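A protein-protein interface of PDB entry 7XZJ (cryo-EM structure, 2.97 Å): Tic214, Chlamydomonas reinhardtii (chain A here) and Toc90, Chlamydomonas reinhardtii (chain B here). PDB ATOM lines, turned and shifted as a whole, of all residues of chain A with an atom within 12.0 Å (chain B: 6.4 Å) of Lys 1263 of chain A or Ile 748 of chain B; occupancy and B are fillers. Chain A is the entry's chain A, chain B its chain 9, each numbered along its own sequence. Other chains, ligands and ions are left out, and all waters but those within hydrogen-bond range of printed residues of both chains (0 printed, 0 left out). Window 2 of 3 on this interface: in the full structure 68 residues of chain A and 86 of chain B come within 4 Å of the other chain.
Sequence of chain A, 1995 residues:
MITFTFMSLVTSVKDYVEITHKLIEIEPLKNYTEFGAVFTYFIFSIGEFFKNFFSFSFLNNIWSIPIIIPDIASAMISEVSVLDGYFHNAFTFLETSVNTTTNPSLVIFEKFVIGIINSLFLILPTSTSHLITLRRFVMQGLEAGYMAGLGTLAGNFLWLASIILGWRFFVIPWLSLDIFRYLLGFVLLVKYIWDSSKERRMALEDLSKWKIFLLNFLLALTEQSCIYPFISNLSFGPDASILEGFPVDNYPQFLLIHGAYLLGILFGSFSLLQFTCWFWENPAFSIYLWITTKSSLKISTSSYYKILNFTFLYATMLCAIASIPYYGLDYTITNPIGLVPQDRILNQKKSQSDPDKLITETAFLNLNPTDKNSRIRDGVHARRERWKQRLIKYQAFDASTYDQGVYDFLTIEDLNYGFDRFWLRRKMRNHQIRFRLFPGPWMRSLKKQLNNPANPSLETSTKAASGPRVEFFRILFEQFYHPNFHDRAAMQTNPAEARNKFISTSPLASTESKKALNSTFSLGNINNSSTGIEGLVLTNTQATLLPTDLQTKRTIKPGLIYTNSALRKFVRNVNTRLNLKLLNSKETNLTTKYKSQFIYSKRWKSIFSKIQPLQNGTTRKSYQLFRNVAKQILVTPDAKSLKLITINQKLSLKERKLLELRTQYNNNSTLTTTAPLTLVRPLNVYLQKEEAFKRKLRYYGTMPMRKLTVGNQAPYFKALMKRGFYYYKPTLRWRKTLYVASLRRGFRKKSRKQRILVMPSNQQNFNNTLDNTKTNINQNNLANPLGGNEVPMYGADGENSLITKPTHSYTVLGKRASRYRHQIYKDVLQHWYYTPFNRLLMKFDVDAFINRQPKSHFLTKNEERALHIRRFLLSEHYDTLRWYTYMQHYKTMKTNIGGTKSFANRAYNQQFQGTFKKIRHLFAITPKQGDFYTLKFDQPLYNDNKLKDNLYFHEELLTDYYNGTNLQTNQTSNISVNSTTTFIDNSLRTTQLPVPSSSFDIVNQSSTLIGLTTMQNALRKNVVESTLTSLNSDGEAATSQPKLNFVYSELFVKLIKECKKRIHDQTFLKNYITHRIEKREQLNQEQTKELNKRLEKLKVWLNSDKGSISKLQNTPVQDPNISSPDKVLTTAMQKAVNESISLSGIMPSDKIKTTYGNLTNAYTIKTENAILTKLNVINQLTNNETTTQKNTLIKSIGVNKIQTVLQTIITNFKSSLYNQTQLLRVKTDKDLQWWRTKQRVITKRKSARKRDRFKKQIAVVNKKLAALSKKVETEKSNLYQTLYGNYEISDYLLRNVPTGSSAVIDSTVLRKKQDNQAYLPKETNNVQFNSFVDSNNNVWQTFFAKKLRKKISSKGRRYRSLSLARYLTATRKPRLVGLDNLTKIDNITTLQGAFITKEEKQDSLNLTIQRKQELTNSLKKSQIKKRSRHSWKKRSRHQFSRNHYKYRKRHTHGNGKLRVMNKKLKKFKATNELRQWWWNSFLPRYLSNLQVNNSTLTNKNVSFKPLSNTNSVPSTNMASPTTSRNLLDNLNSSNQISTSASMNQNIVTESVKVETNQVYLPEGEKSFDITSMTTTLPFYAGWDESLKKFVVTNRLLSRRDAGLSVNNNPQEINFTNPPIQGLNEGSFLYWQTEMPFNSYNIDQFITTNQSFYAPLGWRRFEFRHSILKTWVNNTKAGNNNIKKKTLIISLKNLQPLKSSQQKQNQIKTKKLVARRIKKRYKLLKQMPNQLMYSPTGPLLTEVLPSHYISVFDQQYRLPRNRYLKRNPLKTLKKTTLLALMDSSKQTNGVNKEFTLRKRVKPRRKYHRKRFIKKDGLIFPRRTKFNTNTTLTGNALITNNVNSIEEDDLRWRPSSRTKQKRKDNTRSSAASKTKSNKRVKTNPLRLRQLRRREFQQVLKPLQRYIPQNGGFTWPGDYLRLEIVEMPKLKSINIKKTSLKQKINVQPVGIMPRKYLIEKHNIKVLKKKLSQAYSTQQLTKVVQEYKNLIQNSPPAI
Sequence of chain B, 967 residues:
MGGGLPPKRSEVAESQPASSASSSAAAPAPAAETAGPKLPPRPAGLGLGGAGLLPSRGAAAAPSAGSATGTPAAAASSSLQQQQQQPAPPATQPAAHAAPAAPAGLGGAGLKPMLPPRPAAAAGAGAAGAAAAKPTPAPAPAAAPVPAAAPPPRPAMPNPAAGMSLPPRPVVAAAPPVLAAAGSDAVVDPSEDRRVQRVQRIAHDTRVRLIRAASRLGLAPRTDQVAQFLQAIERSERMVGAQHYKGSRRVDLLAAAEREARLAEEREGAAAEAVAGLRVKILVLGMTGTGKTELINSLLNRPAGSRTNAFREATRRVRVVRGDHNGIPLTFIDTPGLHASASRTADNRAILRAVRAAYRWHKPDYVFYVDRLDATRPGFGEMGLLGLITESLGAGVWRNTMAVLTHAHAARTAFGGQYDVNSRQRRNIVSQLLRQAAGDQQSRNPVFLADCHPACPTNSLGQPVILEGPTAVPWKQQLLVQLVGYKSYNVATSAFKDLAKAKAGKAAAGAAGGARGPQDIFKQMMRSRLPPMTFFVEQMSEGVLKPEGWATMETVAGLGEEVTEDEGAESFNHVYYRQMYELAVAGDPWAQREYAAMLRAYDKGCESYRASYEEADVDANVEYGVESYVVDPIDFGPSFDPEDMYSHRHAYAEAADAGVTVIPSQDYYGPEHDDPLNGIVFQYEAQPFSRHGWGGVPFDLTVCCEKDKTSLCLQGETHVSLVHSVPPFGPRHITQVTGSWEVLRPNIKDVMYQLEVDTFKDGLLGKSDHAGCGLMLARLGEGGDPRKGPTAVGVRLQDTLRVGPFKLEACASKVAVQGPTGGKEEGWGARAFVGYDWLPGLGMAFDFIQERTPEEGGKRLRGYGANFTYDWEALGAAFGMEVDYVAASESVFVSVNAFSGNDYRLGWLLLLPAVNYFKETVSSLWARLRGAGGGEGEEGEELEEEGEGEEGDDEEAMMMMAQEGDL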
ATOM      1  N   ILE A1258      24.145  37.932 -20.349  1.00  0.00           N
ATOM      2  CA  ILE A1258      24.106  36.663 -21.134  1.00  0.00           C
ATOM      3  C   ILE A1258      22.972  35.773 -20.617  1.00  0.00           C
ATOM      4  O   ILE A1258      22.799  34.672 -21.173  1.00  0.00           O
ATOM      5  CB  ILE A1258      25.466  35.950 -21.028  1.00  0.00           C
ATOM      6  CG1 ILE A1258      25.676  35.362 -19.632  1.00  0.00           C
ATOM      7  CG2 ILE A1258      26.594  36.894 -21.406  1.00  0.00           C
ATOM      8  N   ALA A1259      22.227  36.221 -19.601  1.00  0.00           N
ATOM      9  CA  ALA A1259      21.181  35.359 -18.996  1.00  0.00           C
ATOM     10  C   ALA A1259      19.926  35.340 -19.873  1.00  0.00           C
ATOM     11  O   ALA A1259      18.939  35.995 -19.493  1.00  0.00           O
ATOM     12  CB  ALA A1259      20.864  35.846 -17.607  1.00  0.00           C
ATOM     13  N   VAL A1260      19.952  34.599 -20.986  1.00  0.00           N
ATOM     14  CA  VAL A1260      18.779  34.533 -21.910  1.00  0.00           C
ATOM     15  C   VAL A1260      18.551  33.084 -22.349  1.00  0.00           C
ATOM     16  O   VAL A1260      19.551  32.362 -22.532  1.00  0.00           O
ATOM     17  CB  VAL A1260      18.957  35.463 -23.127  1.00  0.00           C
ATOM     18  CG1 VAL A1260      18.626  36.911 -22.800  1.00  0.00           C
ATOM     19  CG2 VAL A1260      20.346  35.352 -23.738  1.00  0.00           C
ATOM     20  N   VAL A1261      17.288  32.670 -22.499  1.00  0.00           N
ATOM     21  CA  VAL A1261      16.993  31.302 -23.023  1.00  0.00           C
ATOM     22  C   VAL A1261      17.468  31.251 -24.478  1.00  0.00           C
ATOM     23  O   VAL A1261      17.351  32.276 -25.172  1.00  0.00           O
ATOM     24  CB  VAL A1261      15.496  30.952 -22.917  1.00  0.00           C
ATOM     25  CG1 VAL A1261      15.126  30.430 -21.539  1.00  0.00           C
ATOM     26  CG2 VAL A1261      14.610  32.128 -23.295  1.00  0.00           C
ATOM     27  N   ASN A1262      18.017  30.113 -24.909  1.00  0.00           N
ATOM     28  CA  ASN A1262      18.542  29.996 -26.295  1.00  0.00           C
ATOM     29  C   ASN A1262      17.397  30.137 -27.305  1.00  0.00           C
ATOM     30  O   ASN A1262      17.597  30.832 -28.319  1.00  0.00           O
ATOM     31  CB  ASN A1262      19.309  28.688 -26.499  1.00  0.00           C
ATOM     32  N   LYS A1263      16.248  29.507 -27.037  1.00  0.00           N
ATOM     33  CA  LYS A1263      15.109  29.530 -27.998  1.00  0.00           C
ATOM     34  C   LYS A1263      14.551  30.948 -28.179  1.00  0.00           C
ATOM     35  O   LYS A1263      14.227  31.297 -29.331  1.00  0.00           O
ATOM     36  CB  LYS A1263      14.029  28.521 -27.594  1.00  0.00           C
ATOM     37  CG  LYS A1263      14.317  27.076 -27.981  1.00  0.00           C
ATOM     38  CD  LYS A1263      13.154  26.140 -27.730  1.00  0.00           C
ATOM     39  CE  LYS A1263      13.355  24.764 -28.328  1.00  0.00           C
ATOM     40  NZ  LYS A1263      14.572  24.104 -27.800  1.00  0.00           N
ATOM     41  N   LYS A1264      14.434  31.732 -27.102  1.00  0.00           N
ATOM     42  CA  LYS A1264      13.803  33.077 -27.212  1.00  0.00           C
ATOM     43  C   LYS A1264      14.752  34.159 -26.683  1.00  0.00           C
ATOM     44  O   LYS A1264      15.971  34.017 -26.884  1.00  0.00           O
ATOM     45  CB  LYS A1264      12.473  33.103 -26.451  1.00  0.00           C
ATOM     46  N   LEU A1265      14.205  35.215 -26.069  1.00  0.00           N
ATOM     47  CA  LEU A1265      15.044  36.294 -25.477  1.00  0.00           C
ATOM     48  C   LEU A1265      14.680  36.510 -24.003  1.00  0.00           C
ATOM     49  O   LEU A1265      15.282  37.407 -23.383  1.00  0.00           O
ATOM     50  CB  LEU A1265      14.841  37.579 -26.286  1.00  0.00           C
ATOM     51  N   ALA A1266      13.730  35.735 -23.467  1.00  0.00           N
ATOM     52  CA  ALA A1266      13.273  35.945 -22.073  1.00  0.00           C
ATOM     53  C   ALA A1266      14.459  35.821 -21.111  1.00  0.00           C
ATOM     54  O   ALA A1266      15.272  34.895 -21.291  1.00  0.00           O
ATOM     55  CB  ALA A1266      12.187  34.953 -21.739  1.00  0.00           C
ATOM     56  N   ALA A1267      14.547  36.720 -20.126  1.00  0.00           N
ATOM     57  CA  ALA A1267      15.691  36.729 -19.181  1.00  0.00           C
ATOM     58  C   ALA A1267      15.614  35.559 -18.194  1.00  0.00           C
ATOM     59  O   ALA A1267      14.496  35.063 -17.949  1.00  0.00           O
ATOM     60  CB  ALA A1267      15.752  38.054 -18.461  1.00  0.00           C
ATOM     61  N   LEU A1268      16.762  35.140 -17.651  1.00  0.00           N
ATOM     62  CA  LEU A1268      16.802  34.037 -16.652  1.00  0.00           C
ATOM     63  C   LEU A1268      17.386  34.582 -15.344  1.00  0.00           C
ATOM     64  O   LEU A1268      18.331  35.389 -15.418  1.00  0.00           O
ATOM     65  CB  LEU A1268      17.662  32.896 -17.202  1.00  0.00           C
ATOM     66  CG  LEU A1268      17.125  32.205 -18.453  1.00  0.00           C
ATOM     67  CD1 LEU A1268      18.120  31.178 -18.972  1.00  0.00           C
ATOM     68  CD2 LEU A1268      15.782  31.548 -18.172  1.00  0.00           C
ATOM     69  N   GLN B 715       8.343  27.005 -21.589  1.00  0.00           N
ATOM     70  CA  GLN B 715       9.746  27.177 -21.133  1.00  0.00           C
ATOM     71  C   GLN B 715       9.760  27.097 -19.607  1.00  0.00           C
ATOM     72  O   GLN B 715       8.967  27.818 -18.979  1.00  0.00           O
ATOM     73  CB  GLN B 715      10.325  28.496 -21.647  1.00  0.00           C
ATOM     74  CG  GLN B 715      10.633  28.481 -23.137  1.00  0.00           C
ATOM     75  CD  GLN B 715      11.245  29.774 -23.615  1.00  0.00           C
ATOM     76  OE1 GLN B 715      11.275  30.772 -22.897  1.00  0.00           O
ATOM     77  NE2 GLN B 715      11.739  29.766 -24.842  1.00  0.00           N
ATOM     78  N   GLU B 742      13.466  24.042 -22.411  1.00  0.00           N
ATOM     79  CA  GLU B 742      12.773  24.957 -23.359  1.00  0.00           C
ATOM     80  C   GLU B 742      12.176  24.143 -24.511  1.00  0.00           C
ATOM     81  O   GLU B 742      12.948  23.422 -25.168  1.00  0.00           O
ATOM     82  CB  GLU B 742      13.761  25.977 -23.924  1.00  0.00           C
ATOM     83  CG  GLU B 742      14.760  26.496 -22.907  1.00  0.00           C
ATOM     84  CD  GLU B 742      15.958  27.205 -23.514  1.00  0.00           C
ATOM     85  OE1 GLU B 742      15.919  27.496 -24.725  1.00  0.00           O
ATOM     86  OE2 GLU B 742      16.931  27.458 -22.776  1.00  0.00           O
ATOM     87  N   VAL B 743      10.864  24.250 -24.747  1.00  0.00           N
ATOM     88  CA  VAL B 743      10.256  23.561 -25.925  1.00  0.00           C
ATOM     89  C   VAL B 743       9.377  24.501 -26.757  1.00  0.00           C
ATOM     90  O   VAL B 743       8.475  25.133 -26.173  1.00  0.00           O
ATOM     91  CB  VAL B 743       9.472  22.302 -25.502  1.00  0.00           C
ATOM     92  CG1 VAL B 743       8.283  22.617 -24.608  1.00  0.00           C
ATOM     93  CG2 VAL B 743       9.049  21.454 -26.692  1.00  0.00           C
ATOM     94  N   LEU B 744       9.640  24.609 -28.063  1.00  0.00           N
ATOM     95  CA  LEU B 744       8.747  25.391 -28.959  1.00  0.00           C
ATOM     96  C   LEU B 744       8.300  24.426 -30.055  1.00  0.00           C
ATOM     97  O   LEU B 744       9.170  24.000 -30.822  1.00  0.00           O
ATOM     98  CB  LEU B 744       9.515  26.580 -29.544  1.00  0.00           C
ATOM     99  CG  LEU B 744       8.703  27.526 -30.427  1.00  0.00           C
ATOM    100  CD1 LEU B 744       7.414  27.942 -29.736  1.00  0.00           C
ATOM    101  CD2 LEU B 744       9.523  28.750 -30.798  1.00  0.00           C
ATOM    102  N   ARG B 745       7.001  24.137 -30.164  1.00  0.00           N
ATOM    103  CA  ARG B 745       6.535  23.091 -31.121  1.00  0.00           C
ATOM    104  C   ARG B 745       6.570  23.566 -32.586  1.00  0.00           C
ATOM    105  O   ARG B 745       7.185  22.837 -33.391  1.00  0.00           O
ATOM    106  CB  ARG B 745       5.160  22.554 -30.709  1.00  0.00           C
ATOM    107  CG  ARG B 745       4.741  21.290 -31.446  1.00  0.00           C
ATOM    108  CD  ARG B 745       5.798  20.205 -31.367  1.00  0.00           C
ATOM    109  NE  ARG B 745       6.126  19.835 -29.997  1.00  0.00           N
ATOM    110  CZ  ARG B 745       7.079  18.974 -29.659  1.00  0.00           C
ATOM    111  NH1 ARG B 745       7.805  18.390 -30.597  1.00  0.00           N
ATOM    112  NH2 ARG B 745       7.304  18.701 -28.387  1.00  0.00           N
ATOM    113  N   PRO B 746       5.976  24.715 -33.014  1.00  0.00           N
ATOM    114  CA  PRO B 746       5.951  25.056 -34.448  1.00  0.00           C
ATOM    115  C   PRO B 746       7.324  25.195 -35.085  1.00  0.00           C
ATOM    116  O   PRO B 746       7.423  25.104 -36.315  1.00  0.00           O
ATOM    117  CB  PRO B 746       5.187  26.386 -34.483  1.00  0.00           C
ATOM    118  CG  PRO B 746       5.369  26.958 -33.130  1.00  0.00           C
ATOM    119  CD  PRO B 746       5.370  25.785 -32.200  1.00  0.00           C
ATOM    120  N   ASN B 747       8.366  25.467 -34.296  1.00  0.00           N
ATOM    121  CA  ASN B 747       9.698  25.728 -34.908  1.00  0.00           C
ATOM    122  C   ASN B 747      10.599  24.497 -34.779  1.00  0.00           C
ATOM    123  O   ASN B 747      11.136  24.057 -35.812  1.00  0.00           O
ATOM    124  CB  ASN B 747      10.356  26.983 -34.330  1.00  0.00           C
ATOM    125  CG  ASN B 747       9.597  28.254 -34.650  1.00  0.00           C
ATOM    126  OD1 ASN B 747       8.522  28.210 -35.244  1.00  0.00           O
ATOM    127  ND2 ASN B 747      10.151  29.391 -34.263  1.00  0.00           N
ATOM    128  N   ILE B 748      10.761  23.965 -33.565  1.00  0.00           N
ATOM    129  CA  ILE B 748      11.692  22.818 -33.346  1.00  0.00           C
ATOM    130  C   ILE B 748      10.888  21.601 -32.874  1.00  0.00           C
ATOM    131  O   ILE B 748      10.059  21.757 -31.965  1.00  0.00           O
ATOM    132  CB  ILE B 748      12.811  23.206 -32.357  1.00  0.00           C
ATOM    133  CG1 ILE B 748      13.508  24.510 -32.756  1.00  0.00           C
ATOM    134  CG2 ILE B 748      13.813  22.072 -32.198  1.00  0.00           C
ATOM    135  CD1 ILE B 748      13.032  25.728 -31.998  1.00  0.00           C
ATOM    136  N   LYS B 749      11.105  20.437 -33.494  1.00  0.00           N
ATOM    137  CA  LYS B 749      10.407  19.194 -33.065  1.00  0.00           C
ATOM    138  C   LYS B 749      11.235  18.521 -31.967  1.00  0.00           C
ATOM    139  O   LYS B 749      11.100  17.294 -31.794  1.00  0.00           O
ATOM    140  CB  LYS B 749      10.206  18.253 -34.256  1.00  0.00           C
ATOM    141  N   ASP B 750      12.044  19.301 -31.245  1.00  0.00           N
ATOM    142  CA  ASP B 750      12.918  18.736 -30.183  1.00  0.00           C
ATOM    143  C   ASP B 750      12.843  19.626 -28.938  1.00  0.00           C
ATOM    144  O   ASP B 750      12.378  20.776 -29.064  1.00  0.00           O
ATOM    145  CB  ASP B 750      14.357  18.586 -30.683  1.00  0.00           C
ATOM    146  N   VAL B 751      13.282  19.110 -27.788  1.00  0.00           N
ATOM    147  CA  VAL B 751      13.275  19.902 -26.522  1.00  0.00           C
ATOM    148  C   VAL B 751      14.726  20.084 -26.073  1.00  0.00           C
ATOM    149  O   VAL B 751      15.470  19.088 -26.081  1.00  0.00           O
ATOM    150  CB  VAL B 751      12.448  19.197 -25.430  1.00  0.00           C
ATOM    151  CG1 VAL B 751      12.287  20.063 -24.190  1.00  0.00           C
ATOM    152  CG2 VAL B 751      11.096  18.730 -25.944  1.00  0.00           C
ATOM    153  N   MET B 752      15.115  21.305 -25.702  1.00  0.00           N
ATOM    154  CA  MET B 752      16.487  21.516 -25.175  1.00  0.00           C
ATOM    155  C   MET B 752      16.453  21.350 -23.655  1.00  0.00           C
ATOM    156  O   MET B 752      15.717  22.109 -22.998  1.00  0.00           O
ATOM    157  CB  MET B 752      16.997  22.919 -25.512  1.00  0.00           C
ATOM    158  CG  MET B 752      18.444  23.146 -25.119  1.00  0.00           C
ATOM    159  SD  MET B 752      18.966  24.849 -25.419  1.00  0.00           S
ATOM    160  CE  MET B 752      18.426  25.060 -27.114  1.00  0.00           C
ATOM    161  N   LEU B 780      20.530  18.576 -26.454  1.00  0.00           N
ATOM    162  CA  LEU B 780      19.355  18.873 -27.316  1.00  0.00           C
ATOM    163  C   LEU B 780      18.666  17.544 -27.645  1.00  0.00           C
ATOM    164  O   LEU B 780      18.898  17.014 -28.747  1.00  0.00           O
ATOM    165  CB  LEU B 780      19.826  19.586 -28.587  1.00  0.00           C
ATOM    166  CG  LEU B 780      18.715  20.125 -29.489  1.00  0.00           C
ATOM    167  CD1 LEU B 780      19.157  21.401 -30.184  1.00  0.00           C
ATOM    168  CD2 LEU B 780      18.296  19.082 -30.512  1.00  0.00           C
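The side-chain carboxylate (OE1) of Glu 742 of chain B is in hydrogen-bond range of the backbone NH (N) of Lys 1263 of chain A (3.1 Å).
N of Asn 1262 of chain A lies within hydrogen-bond range of OE1 of Glu 742 of chain B (3.4 Å).
The backbone NH (N) of Val 1261 of chain A lies within hydrogen-bond range of the backbone carbonyl oxygen (O) of Ala 1266 of chain A, at 3.2 Å.
N of Glu 742 of chain B is in hydrogen-bond range of O of Met 752 of chain B, 3.0 Å away.
Among the printed residues, merely in contact across the chains: Lys 1263 of chain A with Met 752 of chain B, Val 1261 of chain A with Gln 715 of chain B, Val 1261 of chain A with Glu 742 of chain B, Lys 1263 of chain A with Leu 744 of chain B, Lys 1264 of chain A with Gln 715 of chain B, Asn 1262 of chain A with Met 752 of chain B, Lys 1263 of chain A with Gln 715 of chain B and Lys 1263 of chain A with Ile 748 of chain B.
Lys 1263 of chain A touches just these residues of chain B: Gln 715 (3.8 Å), Glu 742 (3.1 Å), Leu 744 (3.7 Å), Ile 748 (3.8 Å) and Met 752 (3.5 Å).
Of chain A, only Val 1261 (3.7 Å), Asn 1262 (3.4 Å) and Lys 1263 (3.1 Å) come within 4 Å of Glu 742 of chain B.
No residue of chain A comes within 4 Å of Val 743 of chain B.
Of chain A, only Lys 1263 comes within 4 Å of Leu 744 of chain B.
No residue of chain A comes within 4 Å of Arg 745 of chain B.
No residue of chain A comes within 4 Å of Pro 746 of chain B.
No residue of chain A comes within 4 Å of Lys 749 of chain B.
No residue of chain A comes within 4 Å of Asp 750 of chain B.
No residue of chain A comes within 4 Å of Val 751 of chain B.
Of chain A, only Asn 1262 and Lys 1263 come within 4 Å of Met 752 of chain B.
Of the printed residues of chain B, Val 1261 of chain A touches Gln 715 and Glu 742.
Of the printed residues of chain A, Gln 715 of chain B touches Val 1261, Lys 1263 and Lys 1264.
The nearest printed residue of chain B that does not touch Lys 1264 of chain A is Glu 742 of chain B (5.1 Å).
Printed residues of chain A that touch a printed residue of chain B: Val 1261, Asn 1262, Lys 1263 and Lys 1264.
Hydrophobic or aromatic side chains of chain A within 4 Å of the printed part of chain B: Val 1261.
Printed residues of chain B that touch a printed residue of chain A: Gln 715, Glu 742, Leu 744, Ile 748 and Met 752.
Hydrophobic or aromatic side chains of chain B that line the printed part of chain A: Ile 748 and Met 752.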
